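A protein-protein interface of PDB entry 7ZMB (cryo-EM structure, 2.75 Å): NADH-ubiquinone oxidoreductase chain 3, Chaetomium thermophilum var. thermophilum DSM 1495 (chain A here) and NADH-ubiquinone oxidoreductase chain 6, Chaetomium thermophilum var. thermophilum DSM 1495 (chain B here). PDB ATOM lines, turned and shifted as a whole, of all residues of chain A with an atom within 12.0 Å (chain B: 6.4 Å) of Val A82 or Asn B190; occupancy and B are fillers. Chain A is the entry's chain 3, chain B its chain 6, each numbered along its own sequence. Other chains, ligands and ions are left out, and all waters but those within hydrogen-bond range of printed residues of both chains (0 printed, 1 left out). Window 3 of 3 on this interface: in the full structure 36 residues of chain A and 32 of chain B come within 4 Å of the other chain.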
ATOM      1  N   LEU A  71       0.065  14.607 -15.305  1.00  0.00           N
ATOM      2  CA  LEU A  71      -0.248  15.395 -14.084  1.00  0.00           C
ATOM      3  C   LEU A  71       0.327  16.805 -14.212  1.00  0.00           C
ATOM      4  O   LEU A  71      -0.327  17.739 -13.720  1.00  0.00           O
ATOM      5  CB  LEU A  71       0.347  14.681 -12.870  1.00  0.00           C
ATOM      6  CG  LEU A  71      -0.001  15.285 -11.510  1.00  0.00           C
ATOM      7  CD1 LEU A  71      -1.383  14.838 -11.056  1.00  0.00           C
ATOM      8  CD2 LEU A  71       1.047  14.927 -10.470  1.00  0.00           C
ATOM      9  N   LEU A  72       1.505  16.949 -14.823  1.00  0.00           N
ATOM     10  CA  LEU A  72       2.144  18.272 -15.037  1.00  0.00           C
ATOM     11  C   LEU A  72       1.390  19.074 -16.105  1.00  0.00           C
ATOM     12  O   LEU A  72       1.761  20.230 -16.291  1.00  0.00           O
ATOM     13  CB  LEU A  72       3.621  18.087 -15.401  1.00  0.00           C
ATOM     14  CG  LEU A  72       4.621  18.499 -14.322  1.00  0.00           C
ATOM     15  CD1 LEU A  72       4.639  17.493 -13.186  1.00  0.00           C
ATOM     16  CD2 LEU A  72       6.013  18.657 -14.906  1.00  0.00           C
ATOM     17  N   LEU A  73       0.458  18.459 -16.841  1.00  0.00           N
ATOM     18  CA  LEU A  73      -0.369  19.178 -17.854  1.00  0.00           C
ATOM     19  C   LEU A  73      -1.729  19.616 -17.296  1.00  0.00           C
ATOM     20  O   LEU A  73      -2.366  20.439 -17.956  1.00  0.00           O
ATOM     21  CB  LEU A  73      -0.565  18.249 -19.052  1.00  0.00           C
ATOM     22  CG  LEU A  73       0.649  18.108 -19.960  1.00  0.00           C
ATOM     23  CD1 LEU A  73       0.344  17.155 -21.100  1.00  0.00           C
ATOM     24  CD2 LEU A  73       1.060  19.473 -20.485  1.00  0.00           C
ATOM     25  N   TYR A  74      -2.097  19.197 -16.083  1.00  0.00           N
ATOM     26  CA  TYR A  74      -3.450  19.469 -15.529  1.00  0.00           C
ATOM     27  C   TYR A  74      -3.533  20.913 -15.023  1.00  0.00           C
ATOM     28  O   TYR A  74      -4.613  21.490 -15.203  1.00  0.00           O
ATOM     29  CB  TYR A  74      -3.791  18.466 -14.422  1.00  0.00           C
ATOM     30  CG  TYR A  74      -4.734  17.354 -14.804  1.00  0.00           C
ATOM     31  CD1 TYR A  74      -4.274  16.201 -15.419  1.00  0.00           C
ATOM     32  CD2 TYR A  74      -6.087  17.444 -14.531  1.00  0.00           C
ATOM     33  CE1 TYR A  74      -5.136  15.176 -15.766  1.00  0.00           C
ATOM     34  CE2 TYR A  74      -6.963  16.428 -14.872  1.00  0.00           C
ATOM     35  CZ  TYR A  74      -6.487  15.289 -15.492  1.00  0.00           C
ATOM     36  OH  TYR A  74      -7.348  14.287 -15.829  1.00  0.00           O
ATOM     37  N   PRO A  75      -2.504  21.535 -14.395  1.00  0.00           N
ATOM     38  CA  PRO A  75      -2.576  22.948 -14.067  1.00  0.00           C
ATOM     39  C   PRO A  75      -2.742  23.814 -15.322  1.00  0.00           C
ATOM     40  O   PRO A  75      -3.444  24.776 -15.211  1.00  0.00           O
ATOM     41  CB  PRO A  75      -1.198  23.233 -13.446  1.00  0.00           C
ATOM     42  CG  PRO A  75      -0.785  21.916 -12.846  1.00  0.00           C
ATOM     43  CD  PRO A  75      -1.278  20.917 -13.864  1.00  0.00           C
ATOM     44  N   PHE A  76      -2.161  23.452 -16.467  1.00  0.00           N
ATOM     45  CA  PHE A  76      -2.398  24.239 -17.673  1.00  0.00           C
ATOM     46  C   PHE A  76      -3.869  24.231 -18.061  1.00  0.00           C
ATOM     47  O   PHE A  76      -4.403  25.248 -18.515  1.00  0.00           O
ATOM     48  CB  PHE A  76      -1.542  23.722 -18.833  1.00  0.00           C
ATOM     49  CG  PHE A  76      -1.801  24.426 -20.126  1.00  0.00           C
ATOM     50  CD1 PHE A  76      -1.171  25.619 -20.413  1.00  0.00           C
ATOM     51  CD2 PHE A  76      -2.697  23.910 -21.047  1.00  0.00           C
ATOM     52  CE1 PHE A  76      -1.428  26.283 -21.594  1.00  0.00           C
ATOM     53  CE2 PHE A  76      -2.957  24.571 -22.224  1.00  0.00           C
ATOM     54  CZ  PHE A  76      -2.316  25.759 -22.499  1.00  0.00           C
ATOM     55  N   ALA A  77      -4.523  23.074 -17.957  1.00  0.00           N
ATOM     56  CA  ALA A  77      -5.938  22.909 -18.375  1.00  0.00           C
ATOM     57  C   ALA A  77      -6.838  23.847 -17.584  1.00  0.00           C
ATOM     58  O   ALA A  77      -7.844  24.311 -18.144  1.00  0.00           O
ATOM     59  CB  ALA A  77      -6.356  21.482 -18.230  1.00  0.00           C
ATOM     60  N   VAL A  78      -6.468  24.110 -16.334  1.00  0.00           N
ATOM     61  CA  VAL A  78      -7.306  24.945 -15.434  1.00  0.00           C
ATOM     62  C   VAL A  78      -6.724  26.357 -15.333  1.00  0.00           C
ATOM     63  O   VAL A  78      -7.104  27.068 -14.412  1.00  0.00           O
ATOM     64  CB  VAL A  78      -7.479  24.256 -14.065  1.00  0.00           C
ATOM     65  CG1 VAL A  78      -8.423  23.070 -14.135  1.00  0.00           C
ATOM     66  CG2 VAL A  78      -6.156  23.872 -13.427  1.00  0.00           C
ATOM     67  N   SER A  79      -5.827  26.734 -16.240  1.00  0.00           N
ATOM     68  CA  SER A  79      -5.179  28.076 -16.208  1.00  0.00           C
ATOM     69  C   SER A  79      -5.044  28.628 -17.620  1.00  0.00           C
ATOM     70  O   SER A  79      -4.279  29.568 -17.779  1.00  0.00           O
ATOM     71  CB  SER A  79      -3.879  28.061 -15.481  1.00  0.00           C
ATOM     72  OG  SER A  79      -3.013  27.088 -16.026  1.00  0.00           O
ATOM     73  N   GLU A  80      -5.731  28.054 -18.601  1.00  0.00           N
ATOM     74  CA  GLU A  80      -5.555  28.453 -20.023  1.00  0.00           C
ATOM     75  C   GLU A  80      -5.817  29.944 -20.263  1.00  0.00           C
ATOM     76  O   GLU A  80      -5.052  30.541 -21.033  1.00  0.00           O
ATOM     77  CB  GLU A  80      -6.445  27.589 -20.907  1.00  0.00           C
ATOM     78  CG  GLU A  80      -5.866  26.230 -21.219  1.00  0.00           C
ATOM     79  CD  GLU A  80      -6.878  25.282 -21.831  1.00  0.00           C
ATOM     80  OE1 GLU A  80      -8.081  25.509 -21.623  1.00  0.00           O
ATOM     81  OE2 GLU A  80      -6.461  24.339 -22.523  1.00  0.00           O
ATOM     82  N   TYR A  81      -6.838  30.528 -19.638  1.00  0.00           N
ATOM     83  CA  TYR A  81      -7.205  31.942 -19.926  1.00  0.00           C
ATOM     84  C   TYR A  81      -6.049  32.878 -19.558  1.00  0.00           C
ATOM     85  O   TYR A  81      -5.847  33.878 -20.244  1.00  0.00           O
ATOM     86  CB  TYR A  81      -8.558  32.289 -19.298  1.00  0.00           C
ATOM     87  CG  TYR A  81      -9.136  33.610 -19.732  1.00  0.00           C
ATOM     88  CD1 TYR A  81      -9.918  33.702 -20.870  1.00  0.00           C
ATOM     89  CD2 TYR A  81      -8.898  34.770 -19.015  1.00  0.00           C
ATOM     90  CE1 TYR A  81     -10.445  34.910 -21.290  1.00  0.00           C
ATOM     91  CE2 TYR A  81      -9.417  35.987 -19.421  1.00  0.00           C
ATOM     92  CZ  TYR A  81     -10.194  36.057 -20.563  1.00  0.00           C
ATOM     93  OH  TYR A  81     -10.717  37.249 -20.971  1.00  0.00           O
ATOM     94  N   VAL A  82      -5.319  32.562 -18.489  1.00  0.00           N
ATOM     95  CA  VAL A  82      -4.138  33.378 -18.100  1.00  0.00           C
ATOM     96  C   VAL A  82      -2.903  32.889 -18.880  1.00  0.00           C
ATOM     97  O   VAL A  82      -2.182  33.759 -19.398  1.00  0.00           O
ATOM     98  CB  VAL A  82      -3.938  33.362 -16.572  1.00  0.00           C
ATOM     99  CG1 VAL A  82      -2.548  33.814 -16.154  1.00  0.00           C
ATOM    100  CG2 VAL A  82      -5.017  34.159 -15.859  1.00  0.00           C
ATOM    101  N   ASN A  83      -2.630  31.587 -18.965  1.00  0.00           N
ATOM    102  CA  ASN A  83      -1.474  31.130 -19.780  1.00  0.00           C
ATOM    103  C   ASN A  83      -1.537  31.737 -21.187  1.00  0.00           C
ATOM    104  O   ASN A  83      -0.505  32.280 -21.623  1.00  0.00           O
ATOM    105  CB  ASN A  83      -1.335  29.608 -19.769  1.00  0.00           C
ATOM    106  CG  ASN A  83      -0.672  29.086 -18.515  1.00  0.00           C
ATOM    107  OD1 ASN A  83       0.344  29.619 -18.081  1.00  0.00           O
ATOM    108  ND2 ASN A  83      -1.231  28.037 -17.938  1.00  0.00           N
ATOM    109  N   SER A  84      -2.684  31.645 -21.866  1.00  0.00           N
ATOM    110  CA  SER A  84      -2.883  32.229 -23.224  1.00  0.00           C
ATOM    111  C   SER A  84      -1.882  31.679 -24.244  1.00  0.00           C
ATOM    112  O   SER A  84      -1.704  30.463 -24.265  1.00  0.00           O
ATOM    113  CB  SER A  84      -2.896  33.729 -23.198  1.00  0.00           C
ATOM    114  OG  SER A  84      -3.318  34.259 -24.446  1.00  0.00           O
ATOM    115  N   ALA A  85      -1.268  32.547 -25.053  1.00  0.00           N
ATOM    116  CA  ALA A  85      -0.325  32.116 -26.117  1.00  0.00           C
ATOM    117  C   ALA A  85       1.052  31.837 -25.529  1.00  0.00           C
ATOM    118  O   ALA A  85       1.604  30.763 -25.795  1.00  0.00           O
ATOM    119  CB  ALA A  85      -0.210  33.193 -27.157  1.00  0.00           C
ATOM    120  N   TYR A  86       1.599  32.799 -24.794  1.00  0.00           N
ATOM    121  CA  TYR A  86       2.925  32.625 -24.212  1.00  0.00           C
ATOM    122  C   TYR A  86       2.995  31.390 -23.317  1.00  0.00           C
ATOM    123  O   TYR A  86       4.001  30.673 -23.317  1.00  0.00           O
ATOM    124  CB  TYR A  86       3.321  33.870 -23.431  1.00  0.00           C
ATOM    125  CG  TYR A  86       4.782  33.880 -23.083  1.00  0.00           C
ATOM    126  CD1 TYR A  86       5.716  34.378 -23.970  1.00  0.00           C
ATOM    127  CD2 TYR A  86       5.229  33.365 -21.881  1.00  0.00           C
ATOM    128  CE1 TYR A  86       7.040  34.374 -23.664  1.00  0.00           C
ATOM    129  CE2 TYR A  86       6.543  33.359 -21.569  1.00  0.00           C
ATOM    130  CZ  TYR A  86       7.447  33.865 -22.461  1.00  0.00           C
ATOM    131  OH  TYR A  86       8.768  33.854 -22.147  1.00  0.00           O
ATOM    132  N   GLY A  87       1.949  31.133 -22.532  1.00  0.00           N
ATOM    133  CA  GLY A  87       1.942  29.942 -21.702  1.00  0.00           C
ATOM    134  C   GLY A  87       1.673  28.684 -22.499  1.00  0.00           C
ATOM    135  O   GLY A  87       2.135  27.603 -22.137  1.00  0.00           O
ATOM    136  N   LEU A  88       0.915  28.809 -23.592  1.00  0.00           N
ATOM    137  CA  LEU A  88       0.669  27.681 -24.482  1.00  0.00           C
ATOM    138  C   LEU A  88       1.961  27.161 -25.093  1.00  0.00           C
ATOM    139  O   LEU A  88       2.136  25.949 -25.252  1.00  0.00           O
ATOM    140  CB  LEU A  88      -0.300  28.089 -25.589  1.00  0.00           C
ATOM    141  CG  LEU A  88      -0.527  27.079 -26.717  1.00  0.00           C
ATOM    142  CD1 LEU A  88      -1.266  25.841 -26.249  1.00  0.00           C
ATOM    143  CD2 LEU A  88      -1.223  27.729 -27.886  1.00  0.00           C
ATOM    144  N   ALA A  89       2.862  28.068 -25.473  1.00  0.00           N
ATOM    145  CA  ALA A  89       4.098  27.656 -26.126  1.00  0.00           C
ATOM    146  C   ALA A  89       4.912  26.735 -25.229  1.00  0.00           C
ATOM    147  O   ALA A  89       5.384  25.681 -25.666  1.00  0.00           O
ATOM    148  CB  ALA A  89       4.912  28.883 -26.516  1.00  0.00           C
ATOM    149  N   ALA A  90       5.072  27.112 -23.961  1.00  0.00           N
ATOM    150  CA  ALA A  90       5.818  26.278 -23.033  1.00  0.00           C
ATOM    151  C   ALA A  90       5.154  24.919 -22.857  1.00  0.00           C
ATOM    152  O   ALA A  90       5.834  23.887 -22.819  1.00  0.00           O
ATOM    153  CB  ALA A  90       5.948  26.988 -21.691  1.00  0.00           C
ATOM    154  N   ALA A  91       3.824  24.904 -22.749  1.00  0.00           N
ATOM    155  CA  ALA A  91       3.101  23.646 -22.625  1.00  0.00           C
ATOM    156  C   ALA A  91       3.307  22.763 -23.853  1.00  0.00           C
ATOM    157  O   ALA A  91       3.405  21.540 -23.731  1.00  0.00           O
ATOM    158  CB  ALA A  91       1.621  23.923 -22.384  1.00  0.00           C
ATOM    159  N   ASN B 182      -8.495  32.147  -7.073  1.00  0.00           N
ATOM    160  CA  ASN B 182      -8.179  30.963  -7.908  1.00  0.00           C
ATOM    161  C   ASN B 182      -8.037  29.731  -7.020  1.00  0.00           C
ATOM    162  O   ASN B 182      -7.879  29.911  -5.810  1.00  0.00           O
ATOM    163  CB  ASN B 182      -6.878  31.141  -8.697  1.00  0.00           C
ATOM    164  CG  ASN B 182      -6.938  32.169  -9.803  1.00  0.00           C
ATOM    165  OD1 ASN B 182      -7.446  33.267  -9.615  1.00  0.00           O
ATOM    166  ND2 ASN B 182      -6.383  31.829 -10.951  1.00  0.00           N
ATOM    167  N   ILE B 185      -4.423  24.800  -7.736  1.00  0.00           N
ATOM    168  CA  ILE B 185      -3.995  24.177  -9.028  1.00  0.00           C
ATOM    169  C   ILE B 185      -3.932  25.252 -10.114  1.00  0.00           C
ATOM    170  O   ILE B 185      -3.021  25.176 -10.950  1.00  0.00           O
ATOM    171  CB  ILE B 185      -4.848  22.955  -9.421  1.00  0.00           C
ATOM    172  CG1 ILE B 185      -4.347  22.344 -10.732  1.00  0.00           C
ATOM    173  CG2 ILE B 185      -6.327  23.304  -9.477  1.00  0.00           C
ATOM    174  CD1 ILE B 185      -5.169  21.192 -11.241  1.00  0.00           C
ATOM    175  N   SER B 186      -4.855  26.217 -10.094  1.00  0.00           N
ATOM    176  CA  SER B 186      -4.826  27.334 -11.069  1.00  0.00           C
ATOM    177  C   SER B 186      -3.717  28.337 -10.713  1.00  0.00           C
ATOM    178  O   SER B 186      -3.091  28.854 -11.638  1.00  0.00           O
ATOM    179  CB  SER B 186      -6.186  27.967 -11.179  1.00  0.00           C
ATOM    180  OG  SER B 186      -6.200  28.951 -12.201  1.00  0.00           O
ATOM    181  N   SER B 187      -3.459  28.570  -9.429  1.00  0.00           N
ATOM    182  CA  SER B 187      -2.405  29.515  -8.982  1.00  0.00           C
ATOM    183  C   SER B 187      -1.044  29.015  -9.442  1.00  0.00           C
ATOM    184  O   SER B 187      -0.192  29.843  -9.800  1.00  0.00           O
ATOM    185  CB  SER B 187      -2.432  29.729  -7.512  1.00  0.00           C
ATOM    186  OG  SER B 187      -3.760  29.941  -7.071  1.00  0.00           O
ATOM    187  N   ILE B 188      -0.876  27.700  -9.463  1.00  0.00           N
ATOM    188  CA  ILE B 188       0.403  27.102  -9.913  1.00  0.00           C
ATOM    189  C   ILE B 188       0.386  27.168 -11.441  1.00  0.00           C
ATOM    190  O   ILE B 188       1.400  27.580 -12.003  1.00  0.00           O
ATOM    191  CB  ILE B 188       0.490  25.654  -9.402  1.00  0.00           C
ATOM    192  CG1 ILE B 188       0.776  25.572  -7.903  1.00  0.00           C
ATOM    193  CG2 ILE B 188       1.490  24.836 -10.207  1.00  0.00           C
ATOM    194  CD1 ILE B 188       0.539  24.209  -7.307  1.00  0.00           C
ATOM    195  N   GLY B 189      -0.743  26.853 -12.076  1.00  0.00           N
ATOM    196  CA  GLY B 189      -0.806  26.977 -13.518  1.00  0.00           C
ATOM    197  C   GLY B 189      -0.566  28.386 -14.013  1.00  0.00           C
ATOM    198  O   GLY B 189      -0.043  28.580 -15.110  1.00  0.00           O
ATOM    199  N   ASN B 190      -0.923  29.389 -13.210  1.00  0.00           N
ATOM    200  CA  ASN B 190      -0.709  30.775 -13.606  1.00  0.00           C
ATOM    201  C   ASN B 190       0.762  31.100 -13.808  1.00  0.00           C
ATOM    202  O   ASN B 190       1.078  32.094 -14.466  1.00  0.00           O
ATOM    203  CB  ASN B 190      -1.308  31.718 -12.566  1.00  0.00           C
ATOM    204  CG  ASN B 190      -2.817  31.830 -12.671  1.00  0.00           C
ATOM    205  OD1 ASN B 190      -3.413  31.474 -13.683  1.00  0.00           O
ATOM    206  ND2 ASN B 190      -3.443  32.326 -11.613  1.00  0.00           N
ATOM    207  N   ILE B 191       1.669  30.299 -13.252  1.00  0.00           N
ATOM    208  CA  ILE B 191       3.097  30.600 -13.300  1.00  0.00           C
ATOM    209  C   ILE B 191       3.961  29.417 -13.706  1.00  0.00           C
ATOM    210  O   ILE B 191       5.139  29.610 -14.048  1.00  0.00           O
ATOM    211  CB  ILE B 191       3.566  31.159 -11.939  1.00  0.00           C
ATOM    212  CG1 ILE B 191       3.348  30.110 -10.860  1.00  0.00           C
ATOM    213  CG2 ILE B 191       2.850  32.447 -11.592  1.00  0.00           C
ATOM    214  CD1 ILE B 191       3.961  30.460  -9.593  1.00  0.00           C
ATOM    215  N   MET B 192       3.454  28.187 -13.699  1.00  0.00           N
ATOM    216  CA  MET B 192       4.273  27.023 -14.012  1.00  0.00           C
ATOM    217  C   MET B 192       4.727  27.009 -15.471  1.00  0.00           C
ATOM    218  O   MET B 192       5.720  26.351 -15.797  1.00  0.00           O
ATOM    219  CB  MET B 192       3.477  25.761 -13.644  1.00  0.00           C
ATOM    220  CG  MET B 192       3.903  24.466 -14.295  1.00  0.00           C
ATOM    221  SD  MET B 192       2.930  23.067 -13.726  1.00  0.00           S
ATOM    222  CE  MET B 192       3.882  22.557 -12.300  1.00  0.00           C
ATOM    223  N   TYR B 193       4.046  27.745 -16.345  1.00  0.00           N
ATOM    224  CA  TYR B 193       4.331  27.726 -17.769  1.00  0.00           C
ATOM    225  C   TYR B 193       4.795  29.063 -18.327  1.00  0.00           C
ATOM    226  O   TYR B 193       5.082  29.150 -19.522  1.00  0.00           O
ATOM    227  CB  TYR B 193       3.095  27.251 -18.547  1.00  0.00           C
ATOM    228  CG  TYR B 193       2.500  25.976 -18.025  1.00  0.00           C
ATOM    229  CD1 TYR B 193       2.959  24.749 -18.459  1.00  0.00           C
ATOM    230  CD2 TYR B 193       1.492  25.998 -17.083  1.00  0.00           C
ATOM    231  CE1 TYR B 193       2.425  23.584 -17.979  1.00  0.00           C
ATOM    232  CE2 TYR B 193       0.953  24.842 -16.597  1.00  0.00           C
ATOM    233  CZ  TYR B 193       1.420  23.634 -17.051  1.00  0.00           C
ATOM    234  OH  TYR B 193       0.870  22.481 -16.563  1.00  0.00           O
ATOM    235  N   THR B 194       5.019  30.046 -17.471  1.00  0.00           N
ATOM    236  CA  THR B 194       5.579  31.332 -17.950  1.00  0.00           C
ATOM    237  C   THR B 194       6.744  31.722 -17.051  1.00  0.00           C
ATOM    238  O   THR B 194       7.880  31.587 -17.507  1.00  0.00           O
ATOM    239  CB  THR B 194       4.507  32.430 -17.992  1.00  0.00           C
ATOM    240  OG1 THR B 194       3.895  32.554 -16.709  1.00  0.00           O
ATOM    241  CG2 THR B 194       3.448  32.184 -19.045  1.00  0.00           C
ATOM    242  N   ASN B 195       6.467  32.137 -15.819  1.00  0.00           N
ATOM    243  CA  ASN B 195       7.504  32.662 -14.891  1.00  0.00           C
ATOM    244  C   ASN B 195       8.560  31.607 -14.550  1.00  0.00           C
ATOM    245  O   ASN B 195       9.731  31.984 -14.427  1.00  0.00           O
ATOM    246  CB  ASN B 195       6.829  33.220 -13.638  1.00  0.00           C
ATOM    247  CG  ASN B 195       5.757  34.249 -13.926  1.00  0.00           C
ATOM    248  OD1 ASN B 195       4.624  33.905 -14.245  1.00  0.00           O
ATOM    249  ND2 ASN B 195       6.100  35.520 -13.799  1.00  0.00           N
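Of the 12 printed residues of chain B, 7 touch a printed residue of chain A.
Printed residues of chain B that touch a printed residue of chain A: Ile B185, Ser B186, Gly B189, Asn B190, Met B192, Tyr B193 and Thr B194.
Hydrophobic or aromatic side chains of chain B that line the printed part of chain A: Ile B185, Met B192 and Tyr B193.
Printed residues of chain A that touch a printed residue of chain B: Leu A72, Leu A73, Pro A75, Phe A76, Val A78, Ser A79, Val A82, Asn A83, Tyr A86, Gly A87 and Ala A90.
Hydrophobic or aromatic side chains of chain A within 4 Å of the printed part of chain B: Pro A75, Phe A76, Val A78, Val A82, Tyr A86 and Ala A90.
Among the printed residues, no Asp or Glu carboxylate lies within 4 Å of a Lys or Arg side-chain nitrogen of the other chain.
Among the printed residues, merely in contact across the chains: Ala A90 with Tyr B193, Val A82 with Asn B190, Asn A83 with Tyr B193, Tyr A86 with Thr B194, Val A78 with Ile B185, Pro A75 with Ile B185, Gly A87 with Tyr B193, Leu A73 with Tyr B193, Pro A75 with Gly B189, Pro A75 with Tyr B193, Gly A87 with Thr B194, Ser A79 with Asn B190, Pro A75 with Met B192 and Leu A72 with Met B192.
Val A82 touches just one residue of chain B: Asn B190.
Asn B190 touches just these residues of chain A: Ser A79 (3.9 Å) and Val A82 (3.5 Å).
No residue of chain A comes within 4 Å of Asn B182.
No residue of chain A comes within 4 Å of Ser B187.
Gly B189 touches three residues of chain A.
No residue of chain A comes within 4 Å of Ile B191.
Of chain A, only Tyr A86 and Gly A87 come within 4 Å of Thr B194.
Of the printed residues of chain B, Ser A79 touches Gly B189 and Asn B190.
Of the printed residues of chain B, Gly A87 touches Tyr B193 (3.7 Å) and Thr B194 (3.8 Å).
The nearest residue of chain B that does not touch Val A82 is Asn B182 (5.6 Å).
The nearest residue of chain A that does not touch Asn B190 is Asn A83 (4.4 Å).
The side-chain hydroxyl (OH) of Tyr B193 is in hydrogen-bond range of the backbone carbonyl oxygen (O) of Leu A72, at 2.4 Å.
N of Phe A76 lies within hydrogen-bond range of OH of Tyr B193.
O of Val A78 sits at hydrogen-bond distance from OG of Ser B186 (3.0 Å).
The backbone carbonyl oxygen (O) of Gly B189 lies close to the side-chain hydroxyl (OG) of Ser A79 (3.4 Å).
O of Gly B189 sits at hydrogen-bond distance from ND2 of Asn A83.
O of Pro A75 sits at hydrogen-bond distance from OG of Ser A79 (2.5 Å).
The side-chain hydroxyl (OG) of Ser A79 lies within hydrogen-bond range of the side-chain amide nitrogen (ND2) of Asn A83, 2.8 Å away.
ND2 of Asn B182 is in hydrogen-bond range of OG of Ser B186, at 3.1 Å.
ND2 of Asn B182 sits close to ND2 of Asn B190 (3.1 Å).
SD of Met B192 lies within hydrogen-bond range of OH of Tyr B193 (3.6 Å).
The side-chain amide oxygen (OD1) of Asn B195 sits at hydrogen-bond distance from the side-chain hydroxyl (OG1) of Thr B194, 2.9 Å away.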
